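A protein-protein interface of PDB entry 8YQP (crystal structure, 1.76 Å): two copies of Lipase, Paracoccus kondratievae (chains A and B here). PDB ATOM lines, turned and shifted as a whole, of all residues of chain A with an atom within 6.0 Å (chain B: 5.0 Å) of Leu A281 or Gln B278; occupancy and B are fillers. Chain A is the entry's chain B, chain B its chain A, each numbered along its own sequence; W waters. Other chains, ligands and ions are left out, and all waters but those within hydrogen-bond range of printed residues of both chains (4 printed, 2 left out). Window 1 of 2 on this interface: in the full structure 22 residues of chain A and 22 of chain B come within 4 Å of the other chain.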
ATOM      1  N   VAL A  91      22.713  10.012   5.029  1.00  0.00           N
ATOM      2  CA  VAL A  91      21.377  10.535   4.745  1.00  0.00           C
ATOM      3  C   VAL A  91      20.311   9.644   5.370  1.00  0.00           C
ATOM      4  O   VAL A  91      19.406  10.123   6.064  1.00  0.00           O
ATOM      5  CB  VAL A  91      21.164  10.683   3.225  1.00  0.00           C
ATOM      6  CG1 VAL A  91      19.706  11.012   2.932  1.00  0.00           C
ATOM      7  CG2 VAL A  91      22.069  11.757   2.693  1.00  0.00           C
ATOM      8  N   GLU A  94      20.282   9.943   9.144  1.00  0.00           N
ATOM      9  CA  GLU A  94      19.650  11.167   9.625  1.00  0.00           C
ATOM     10  C   GLU A  94      18.140  11.147   9.427  1.00  0.00           C
ATOM     11  O   GLU A  94      17.408  11.725  10.241  1.00  0.00           O
ATOM     12  CB  GLU A  94      20.269  12.402   8.961  1.00  0.00           C
ATOM     13  CG  GLU A  94      21.712  12.678   9.457  1.00  0.00           C
ATOM     14  CD  GLU A  94      22.319  13.961   8.902  1.00  0.00           C
ATOM     15  OE1 GLU A  94      21.560  14.807   8.363  1.00  0.00           O
ATOM     16  OE2 GLU A  94      23.564  14.108   8.999  1.00  0.00           O
ATOM     17  N   ILE A  95      17.643  10.488   8.378  1.00  0.00           N
ATOM     18  CA  ILE A  95      16.198  10.313   8.256  1.00  0.00           C
ATOM     19  C   ILE A  95      15.669   9.528   9.446  1.00  0.00           C
ATOM     20  O   ILE A  95      14.675   9.905  10.077  1.00  0.00           O
ATOM     21  CB  ILE A  95      15.839   9.621   6.934  1.00  0.00           C
ATOM     22  CG1 ILE A  95      16.085  10.584   5.773  1.00  0.00           C
ATOM     23  CG2 ILE A  95      14.367   9.214   6.950  1.00  0.00           C
ATOM     24  CD1 ILE A  95      16.075   9.881   4.430  1.00  0.00           C
ATOM     25  N   ALA A  98      15.896  11.687  12.819  1.00  0.00           N
ATOM     26  CA  ALA A  98      15.023  12.845  12.889  1.00  0.00           C
ATOM     27  C   ALA A  98      13.565  12.426  13.002  1.00  0.00           C
ATOM     28  O   ALA A  98      12.812  13.005  13.784  1.00  0.00           O
ATOM     29  CB  ALA A  98      15.242  13.744  11.663  1.00  0.00           C
ATOM     30  N   THR A  99      13.149  11.426  12.221  1.00  0.00           N
ATOM     31  CA  THR A  99      11.739  11.060  12.141  1.00  0.00           C
ATOM     32  C   THR A  99      11.341  10.016  13.178  1.00  0.00           C
ATOM     33  O   THR A  99      10.155   9.900  13.505  1.00  0.00           O
ATOM     34  CB  THR A  99      11.397  10.518  10.738  1.00  0.00           C
ATOM     35  OG1 THR A  99      12.062   9.266  10.508  1.00  0.00           O
ATOM     36  CG2 THR A  99      11.844  11.491   9.617  1.00  0.00           C
ATOM     37  N   ARG A 267      24.562  19.703   2.601  1.00  0.00           N
ATOM     38  CA  ARG A 267      23.746  20.166   3.718  1.00  0.00           C
ATOM     39  C   ARG A 267      24.573  20.557   4.939  1.00  0.00           C
ATOM     40  O   ARG A 267      24.062  21.284   5.804  1.00  0.00           O
ATOM     41  CB  ARG A 267      22.702  19.119   4.117  1.00  0.00           C
ATOM     42  CG  ARG A 267      23.255  17.801   4.652  1.00  0.00           C
ATOM     43  CD  ARG A 267      22.128  16.766   4.862  1.00  0.00           C
ATOM     44  NE  ARG A 267      22.612  15.594   5.591  1.00  0.00           N
ATOM     45  CZ  ARG A 267      23.511  14.735   5.122  1.00  0.00           C
ATOM     46  NH1 ARG A 267      23.942  14.792   3.861  1.00  0.00           N
ATOM     47  NH2 ARG A 267      23.990  13.790   5.934  1.00  0.00           N
ATOM     48  N   ARG A 274      20.838  22.796   3.498  1.00  0.00           N
ATOM     49  CA  ARG A 274      20.375  22.340   4.810  1.00  0.00           C
ATOM     50  C   ARG A 274      18.879  22.576   4.956  1.00  0.00           C
ATOM     51  O   ARG A 274      18.153  21.682   5.398  1.00  0.00           O
ATOM     52  CB  ARG A 274      21.174  23.049   5.904  1.00  0.00           C
ATOM     53  CG  ARG A 274      20.673  22.798   7.349  1.00  0.00           C
ATOM     54  CD  ARG A 274      21.548  23.535   8.353  1.00  0.00           C
ATOM     55  NE  ARG A 274      21.495  24.987   8.198  1.00  0.00           N
ATOM     56  CZ  ARG A 274      20.491  25.748   8.606  1.00  0.00           C
ATOM     57  NH1 ARG A 274      19.458  25.239   9.259  1.00  0.00           N
ATOM     58  NH2 ARG A 274      20.541  27.060   8.387  1.00  0.00           N
ATOM     59  N   SER A 276      16.771  22.647   2.548  1.00  0.00           N
ATOM     60  CA  SER A 276      16.088  21.705   1.670  1.00  0.00           C
ATOM     61  C   SER A 276      15.923  20.346   2.346  1.00  0.00           C
ATOM     62  O   SER A 276      14.842  19.742   2.302  1.00  0.00           O
ATOM     63  CB  SER A 276      16.847  21.552   0.359  1.00  0.00           C
ATOM     64  OG  SER A 276      16.023  20.861  -0.551  1.00  0.00           O
ATOM     65  N   PHE A 277      16.986  19.850   2.988  1.00  0.00           N
ATOM     66  CA  PHE A 277      16.882  18.567   3.677  1.00  0.00           C
ATOM     67  C   PHE A 277      15.920  18.645   4.853  1.00  0.00           C
ATOM     68  O   PHE A 277      15.206  17.678   5.140  1.00  0.00           O
ATOM     69  CB  PHE A 277      18.266  18.091   4.128  1.00  0.00           C
ATOM     70  CG  PHE A 277      18.287  16.660   4.577  1.00  0.00           C
ATOM     71  CD1 PHE A 277      17.937  15.645   3.702  1.00  0.00           C
ATOM     72  CD2 PHE A 277      18.661  16.332   5.871  1.00  0.00           C
ATOM     73  CE1 PHE A 277      17.945  14.323   4.101  1.00  0.00           C
ATOM     74  CE2 PHE A 277      18.692  15.005   6.274  1.00  0.00           C
ATOM     75  CZ  PHE A 277      18.340  13.999   5.376  1.00  0.00           C
ATOM     76  N   GLN A 278      15.857  19.797   5.520  1.00  0.00           N
ATOM     77  CA  GLN A 278      14.853  19.989   6.562  1.00  0.00           C
ATOM     78  C   GLN A 278      13.441  19.877   5.992  1.00  0.00           C
ATOM     79  O   GLN A 278      12.557  19.271   6.609  1.00  0.00           O
ATOM     80  CB  GLN A 278      15.072  21.341   7.254  1.00  0.00           C
ATOM     81  CG  GLN A 278      16.354  21.351   8.086  1.00  0.00           C
ATOM     82  CD  GLN A 278      16.756  22.702   8.643  1.00  0.00           C
ATOM     83  OE1 GLN A 278      17.762  22.805   9.364  1.00  0.00           O
ATOM     84  NE2 GLN A 278      15.961  23.743   8.359  1.00  0.00           N
ATOM     85  N   ALA A 279      13.209  20.438   4.801  1.00  0.00           N
ATOM     86  CA  ALA A 279      11.903  20.306   4.160  1.00  0.00           C
ATOM     87  C   ALA A 279      11.645  18.880   3.691  1.00  0.00           C
ATOM     88  O   ALA A 279      10.494  18.417   3.685  1.00  0.00           O
ATOM     89  CB  ALA A 279      11.814  21.270   2.974  1.00  0.00           C
ATOM     90  N   ILE A 280      12.695  18.184   3.248  1.00  0.00           N
ATOM     91  CA  ILE A 280      12.548  16.797   2.814  1.00  0.00           C
ATOM     92  C   ILE A 280      12.181  15.906   3.997  1.00  0.00           C
ATOM     93  O   ILE A 280      11.312  15.039   3.888  1.00  0.00           O
ATOM     94  CB  ILE A 280      13.834  16.321   2.119  1.00  0.00           C
ATOM     95  CG1 ILE A 280      13.928  16.937   0.717  1.00  0.00           C
ATOM     96  CG2 ILE A 280      13.894  14.777   2.031  1.00  0.00           C
ATOM     97  CD1 ILE A 280      15.360  17.030   0.148  1.00  0.00           C
ATOM     98  N   LEU A 281      12.837  16.107   5.138  1.00  0.00           N
ATOM     99  CA  LEU A 281      12.480  15.365   6.351  1.00  0.00           C
ATOM    100  C   LEU A 281      11.042  15.637   6.787  1.00  0.00           C
ATOM    101  O   LEU A 281      10.331  14.715   7.216  1.00  0.00           O
ATOM    102  CB  LEU A 281      13.447  15.721   7.483  1.00  0.00           C
ATOM    103  CG  LEU A 281      14.878  15.270   7.214  1.00  0.00           C
ATOM    104  CD1 LEU A 281      15.857  15.871   8.223  1.00  0.00           C
ATOM    105  CD2 LEU A 281      14.942  13.755   7.252  1.00  0.00           C
ATOM    106  N   SER A 282      10.605  16.901   6.732  1.00  0.00           N
ATOM    107  CA  SER A 282       9.246  17.223   7.153  1.00  0.00           C
ATOM    108  C   SER A 282       8.211  16.618   6.212  1.00  0.00           C
ATOM    109  O   SER A 282       7.128  16.229   6.664  1.00  0.00           O
ATOM    110  CB  SER A 282       9.050  18.743   7.248  1.00  0.00           C
ATOM    111  OG  SER A 282       9.999  19.347   8.110  1.00  0.00           O
ATOM    112  N   ALA A 283       8.518  16.540   4.906  1.00  0.00           N
ATOM    113  CA  ALA A 283       7.602  15.912   3.960  1.00  0.00           C
ATOM    114  C   ALA A 283       7.490  14.418   4.231  1.00  0.00           C
ATOM    115  O   ALA A 283       6.388  13.856   4.205  1.00  0.00           O
ATOM    116  CB  ALA A 283       8.066  16.167   2.524  1.00  0.00           C
ATOM    117  N   ILE A 284       8.621  13.767   4.512  1.00  0.00           N
ATOM    118  CA  ILE A 284       8.606  12.360   4.911  1.00  0.00           C
ATOM    119  C   ILE A 284       7.707  12.164   6.126  1.00  0.00           C
ATOM    120  O   ILE A 284       6.790  11.339   6.112  1.00  0.00           O
ATOM    121  CB  ILE A 284      10.033  11.868   5.188  1.00  0.00           C
ATOM    122  CG1 ILE A 284      10.825  11.799   3.887  1.00  0.00           C
ATOM    123  CG2 ILE A 284      10.005  10.488   5.829  1.00  0.00           C
ATOM    124  CD1 ILE A 284      12.256  11.440   4.091  1.00  0.00           C
ATOM    125  N   MET A 285       7.960  12.929   7.197  1.00  0.00           N
ATOM    126  CA  MET A 285       7.122  12.834   8.397  1.00  0.00           C
ATOM    127  C   MET A 285       5.660  13.109   8.096  1.00  0.00           C
ATOM    128  O   MET A 285       4.771  12.478   8.674  1.00  0.00           O
ATOM    129  CB  MET A 285       7.615  13.792   9.484  1.00  0.00           C
ATOM    130  CG  MET A 285       7.109  13.413  10.859  1.00  0.00           C
ATOM    131  SD  MET A 285       8.123  12.165  11.647  1.00  0.00           S
ATOM    132  CE  MET A 285       6.989  10.788  11.719  1.00  0.00           C
ATOM    133  N   ARG A 286       5.394  14.062   7.209  1.00  0.00           N
ATOM    134  CA  ARG A 286       4.024  14.424   6.884  1.00  0.00           C
ATOM    135  C   ARG A 286       3.274  13.237   6.296  1.00  0.00           C
ATOM    136  O   ARG A 286       2.136  12.949   6.691  1.00  0.00           O
ATOM    137  CB  ARG A 286       4.037  15.599   5.908  1.00  0.00           C
ATOM    138  CG  ARG A 286       2.716  16.250   5.672  1.00  0.00           C
ATOM    139  CD  ARG A 286       2.898  17.717   5.300  1.00  0.00           C
ATOM    140  NE  ARG A 286       3.636  17.892   4.051  1.00  0.00           N
ATOM    141  CZ  ARG A 286       4.837  18.452   3.930  1.00  0.00           C
ATOM    142  NH1 ARG A 286       5.487  18.939   4.975  1.00  0.00           N
ATOM    143  NH2 ARG A 286       5.387  18.548   2.720  1.00  0.00           N
ATOM    144  N   ARG B 274      22.622  20.434  14.314  1.00  0.00           N
ATOM    145  CA  ARG B 274      21.848  20.338  13.083  1.00  0.00           C
ATOM    146  C   ARG B 274      20.881  19.153  13.127  1.00  0.00           C
ATOM    147  O   ARG B 274      19.712  19.285  12.753  1.00  0.00           O
ATOM    148  CB  ARG B 274      22.802  20.239  11.880  1.00  0.00           C
ATOM    149  CG  ARG B 274      22.077  20.232  10.566  1.00  0.00           C
ATOM    150  CD  ARG B 274      22.997  20.047   9.324  1.00  0.00           C
ATOM    151  NE  ARG B 274      23.961  18.965   9.487  1.00  0.00           N
ATOM    152  CZ  ARG B 274      23.671  17.714   9.178  1.00  0.00           C
ATOM    153  NH1 ARG B 274      22.458  17.382   8.766  1.00  0.00           N
ATOM    154  NH2 ARG B 274      24.605  16.768   9.317  1.00  0.00           N
ATOM    155  N   ARG B 275      21.351  17.968  13.568  1.00  0.00           N
ATOM    156  CA  ARG B 275      20.431  16.832  13.671  1.00  0.00           C
ATOM    157  C   ARG B 275      19.338  17.081  14.703  1.00  0.00           C
ATOM    158  O   ARG B 275      18.196  16.630  14.530  1.00  0.00           O
ATOM    159  CB  ARG B 275      21.192  15.542  14.007  1.00  0.00           C
ATOM    160  CG  ARG B 275      22.010  15.022  12.807  1.00  0.00           C
ATOM    161  CD  ARG B 275      22.579  13.645  13.068  1.00  0.00           C
ATOM    162  NE  ARG B 275      23.099  13.517  14.423  1.00  0.00           N
ATOM    163  CZ  ARG B 275      24.391  13.513  14.725  1.00  0.00           C
ATOM    164  NH1 ARG B 275      25.326  13.659  13.792  1.00  0.00           N
ATOM    165  NH2 ARG B 275      24.757  13.372  15.996  1.00  0.00           N
ATOM    166  N   SER B 276      19.671  17.764  15.798  1.00  0.00           N
ATOM    167  CA  SER B 276      18.659  18.041  16.820  1.00  0.00           C
ATOM    168  C   SER B 276      17.544  18.898  16.248  1.00  0.00           C
ATOM    169  O   SER B 276      16.359  18.643  16.493  1.00  0.00           O
ATOM    170  CB  SER B 276      19.284  18.734  18.032  1.00  0.00           C
ATOM    171  OG  SER B 276      18.334  18.822  19.127  1.00  0.00           O
ATOM    172  N   PHE B 277      17.898  19.909  15.459  1.00  0.00           N
ATOM    173  CA  PHE B 277      16.852  20.750  14.886  1.00  0.00           C
ATOM    174  C   PHE B 277      16.040  19.980  13.851  1.00  0.00           C
ATOM    175  O   PHE B 277      14.825  20.196  13.737  1.00  0.00           O
ATOM    176  CB  PHE B 277      17.464  22.021  14.280  1.00  0.00           C
ATOM    177  CG  PHE B 277      16.439  23.068  13.876  1.00  0.00           C
ATOM    178  CD1 PHE B 277      15.543  23.579  14.807  1.00  0.00           C
ATOM    179  CD2 PHE B 277      16.384  23.543  12.577  1.00  0.00           C
ATOM    180  CE1 PHE B 277      14.609  24.526  14.448  1.00  0.00           C
ATOM    181  CE2 PHE B 277      15.453  24.517  12.218  1.00  0.00           C
ATOM    182  CZ  PHE B 277      14.567  24.994  13.151  1.00  0.00           C
ATOM    183  N   GLN B 278      16.688  19.062  13.123  1.00  0.00           N
ATOM    184  CA  GLN B 278      15.973  18.164  12.223  1.00  0.00           C
ATOM    185  C   GLN B 278      14.927  17.349  12.975  1.00  0.00           C
ATOM    186  O   GLN B 278      13.813  17.140  12.478  1.00  0.00           O
ATOM    187  CB  GLN B 278      16.988  17.274  11.496  1.00  0.00           C
ATOM    188  CG  GLN B 278      17.769  18.116  10.441  1.00  0.00           C
ATOM    189  CD  GLN B 278      18.926  17.434   9.760  1.00  0.00           C
ATOM    190  OE1 GLN B 278      19.568  18.039   8.879  1.00  0.00           O
ATOM    191  NE2 GLN B 278      19.207  16.184  10.127  1.00  0.00           N
ATOM    192  N   ALA B 279      15.262  16.903  14.184  1.00  0.00           N
ATOM    193  CA  ALA B 279      14.319  16.152  15.008  1.00  0.00           C
ATOM    194  C   ALA B 279      13.218  17.050  15.556  1.00  0.00           C
ATOM    195  O   ALA B 279      12.063  16.630  15.670  1.00  0.00           O
ATOM    196  CB  ALA B 279      15.066  15.475  16.156  1.00  0.00           C
ATOM    197  N   ILE B 280      13.566  18.289  15.904  1.00  0.00           N
ATOM    198  CA  ILE B 280      12.574  19.254  16.380  1.00  0.00           C
ATOM    199  C   ILE B 280      11.551  19.568  15.295  1.00  0.00           C
ATOM    200  O   ILE B 280      10.337  19.583  15.540  1.00  0.00           O
ATOM    201  CB  ILE B 280      13.280  20.520  16.900  1.00  0.00           C
ATOM    202  CG1 ILE B 280      13.889  20.219  18.283  1.00  0.00           C
ATOM    203  CG2 ILE B 280      12.322  21.698  16.992  1.00  0.00           C
ATOM    204  CD1 ILE B 280      15.079  21.100  18.624  1.00  0.00           C
ATOM    205  N   LEU B 281      12.027  19.838  14.075  1.00  0.00           N
ATOM    206  CA  LEU B 281      11.121  20.069  12.958  1.00  0.00           C
ATOM    207  C   LEU B 281      10.186  18.881  12.750  1.00  0.00           C
ATOM    208  O   LEU B 281       8.978  19.054  12.543  1.00  0.00           O
ATOM    209  CB  LEU B 281      11.952  20.328  11.696  1.00  0.00           C
ATOM    210  CG  LEU B 281      12.657  21.668  11.688  1.00  0.00           C
ATOM    211  CD1 LEU B 281      13.492  21.757  10.416  1.00  0.00           C
ATOM    212  CD2 LEU B 281      11.618  22.801  11.702  1.00  0.00           C
ATOM    213  N   SER B 282      10.730  17.661  12.803  1.00  0.00           N
ATOM    214  CA  SER B 282       9.909  16.468  12.615  1.00  0.00           C
ATOM    215  C   SER B 282       8.862  16.320  13.716  1.00  0.00           C
ATOM    216  O   SER B 282       7.731  15.906  13.439  1.00  0.00           O
ATOM    217  CB  SER B 282      10.797  15.223  12.546  1.00  0.00           C
ATOM    218  OG  SER B 282      11.563  15.213  11.355  1.00  0.00           O
HETATM  219  O   HOH W   1      25.308  13.544  11.017  1.00  0.00           O
HETATM  220  O   HOH W   2      19.953  19.694   6.990  1.00  0.00           O
HETATM  221  O   HOH W   3      11.602  13.734  16.178  1.00  0.00           O
HETATM  222  O   HOH W   4      19.258  21.878  11.308  1.00  0.00           O
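Printed residues of chain A that touch a printed residue of chain B: Glu A94, Ala A98, Arg A267, Arg A274, Phe A277, Gln A278, Leu A281 and Met A285. Hydrophobic or aromatic side chains of chain A within 4 Å of the printed part of chain B: Ala A98, Phe A277, Leu A281 and Met A285. Of the 9 printed residues of chain B, 7 touch a printed residue of chain A. Among the printed residues, Asp or Glu carboxylates within 4 Å of a Lys or Arg side-chain nitrogen of the other chain: Glu A94 with Arg B274 (2.8 Å).
Water W2 bridges OE1 of Gln B278 (2.5 Å) and O of Arg A274 (3.1 Å). Water W4 lies within hydrogen-bond range of the side-chain amide oxygen (OE1) of Gln A278 (2.6 Å) and the backbone carbonyl oxygen (O) of Arg B274 (3.0 Å). Water W1 bridges OE2 of Glu A94 (2.7 Å) and NH1 of Arg B275 (2.8 Å). Water W3 bridges the backbone carbonyl oxygen of Ala A98 (2.8 Å) and the backbone carbonyl oxygen of Ala B279 (3.0 Å).
The side-chain hydroxyl (OG) of Ser A282 is in hydrogen-bond range of the backbone carbonyl oxygen (O) of Gln A278, at 3.0 Å. NH1 of Arg B274 is in hydrogen-bond range of OE1 of Gln B278, at 3.0 Å. OE1 of Glu A94 is in salt-bridge range of NE of Arg A267, 3.1 Å away. The backbone carbonyl oxygen of Gln B278 is in hydrogen-bond range of the side-chain hydroxyl of Ser B282, at 3.2 Å. NH1 of Arg A274 sits at hydrogen-bond distance from OE1 of Gln A278 (3.0 Å).
Arg A274 touches its own counterpart, Arg B274. Phe A277 touches Gln B278, and with the chains exchanged Gln A278 touches Phe B277. Gln A278 touches Leu B281, and with the chains exchanged Leu A281 touches Gln B278. Positions printed for both chains: 274, 276, 277, 278, 279, 280, 281 and 282. Of the 13 pairs that touch across the chains among the printed residues, 5 have their exchanged pair printed and touching as well.
The side-chain amide nitrogen (NE2) of Gln B278 is in hydrogen-bond range of the side-chain carboxylate (OE1) of Glu A94, at 3.2 Å. The guanidinium group of Arg B274 is in salt-bridge range of the side-chain carboxylate of Glu A94 (2.8 Å).
Of chain B, only Gln B278 comes within 4 Å of Leu A281. Gln B278 touches four residues of chain A. Of the printed residues of chain A, Leu B281 touches Gln A278 (3.6 Å). Printed residues of chain A within 4 Å of Ser B282: Ala A98 (3.2 Å) and Met A285 (3.6 Å). Printed residues of chain A within 4 Å of Ala B279: Ala A98. Of the printed residues of chain A, Arg B275 touches Glu A94 (3.8 Å). Arg A286 touches none of the printed residues of chain B. Ile A95 touches none of the printed residues of chain B.
Among the printed residues, pairs that only touch across the chains: Glu A94 with Arg B275 (3.8 Å), Ala A98 with Gln B278 (3.8 Å), Ala A98 with Ala B279 (3.7 Å), Ala A98 with Ser B282 (3.2 Å), Arg A267 with Arg B274 (3.6 Å), Arg A274 with Arg B274 (3.9 Å), Phe A277 with Gln B278 (3.6 Å), Gln A278 with Phe B277 (3.6 Å), Gln A278 with Leu B281 (3.6 Å), Leu A281 with Gln B278 (3.7 Å) and Met A285 with Ser B282 (3.6 Å).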
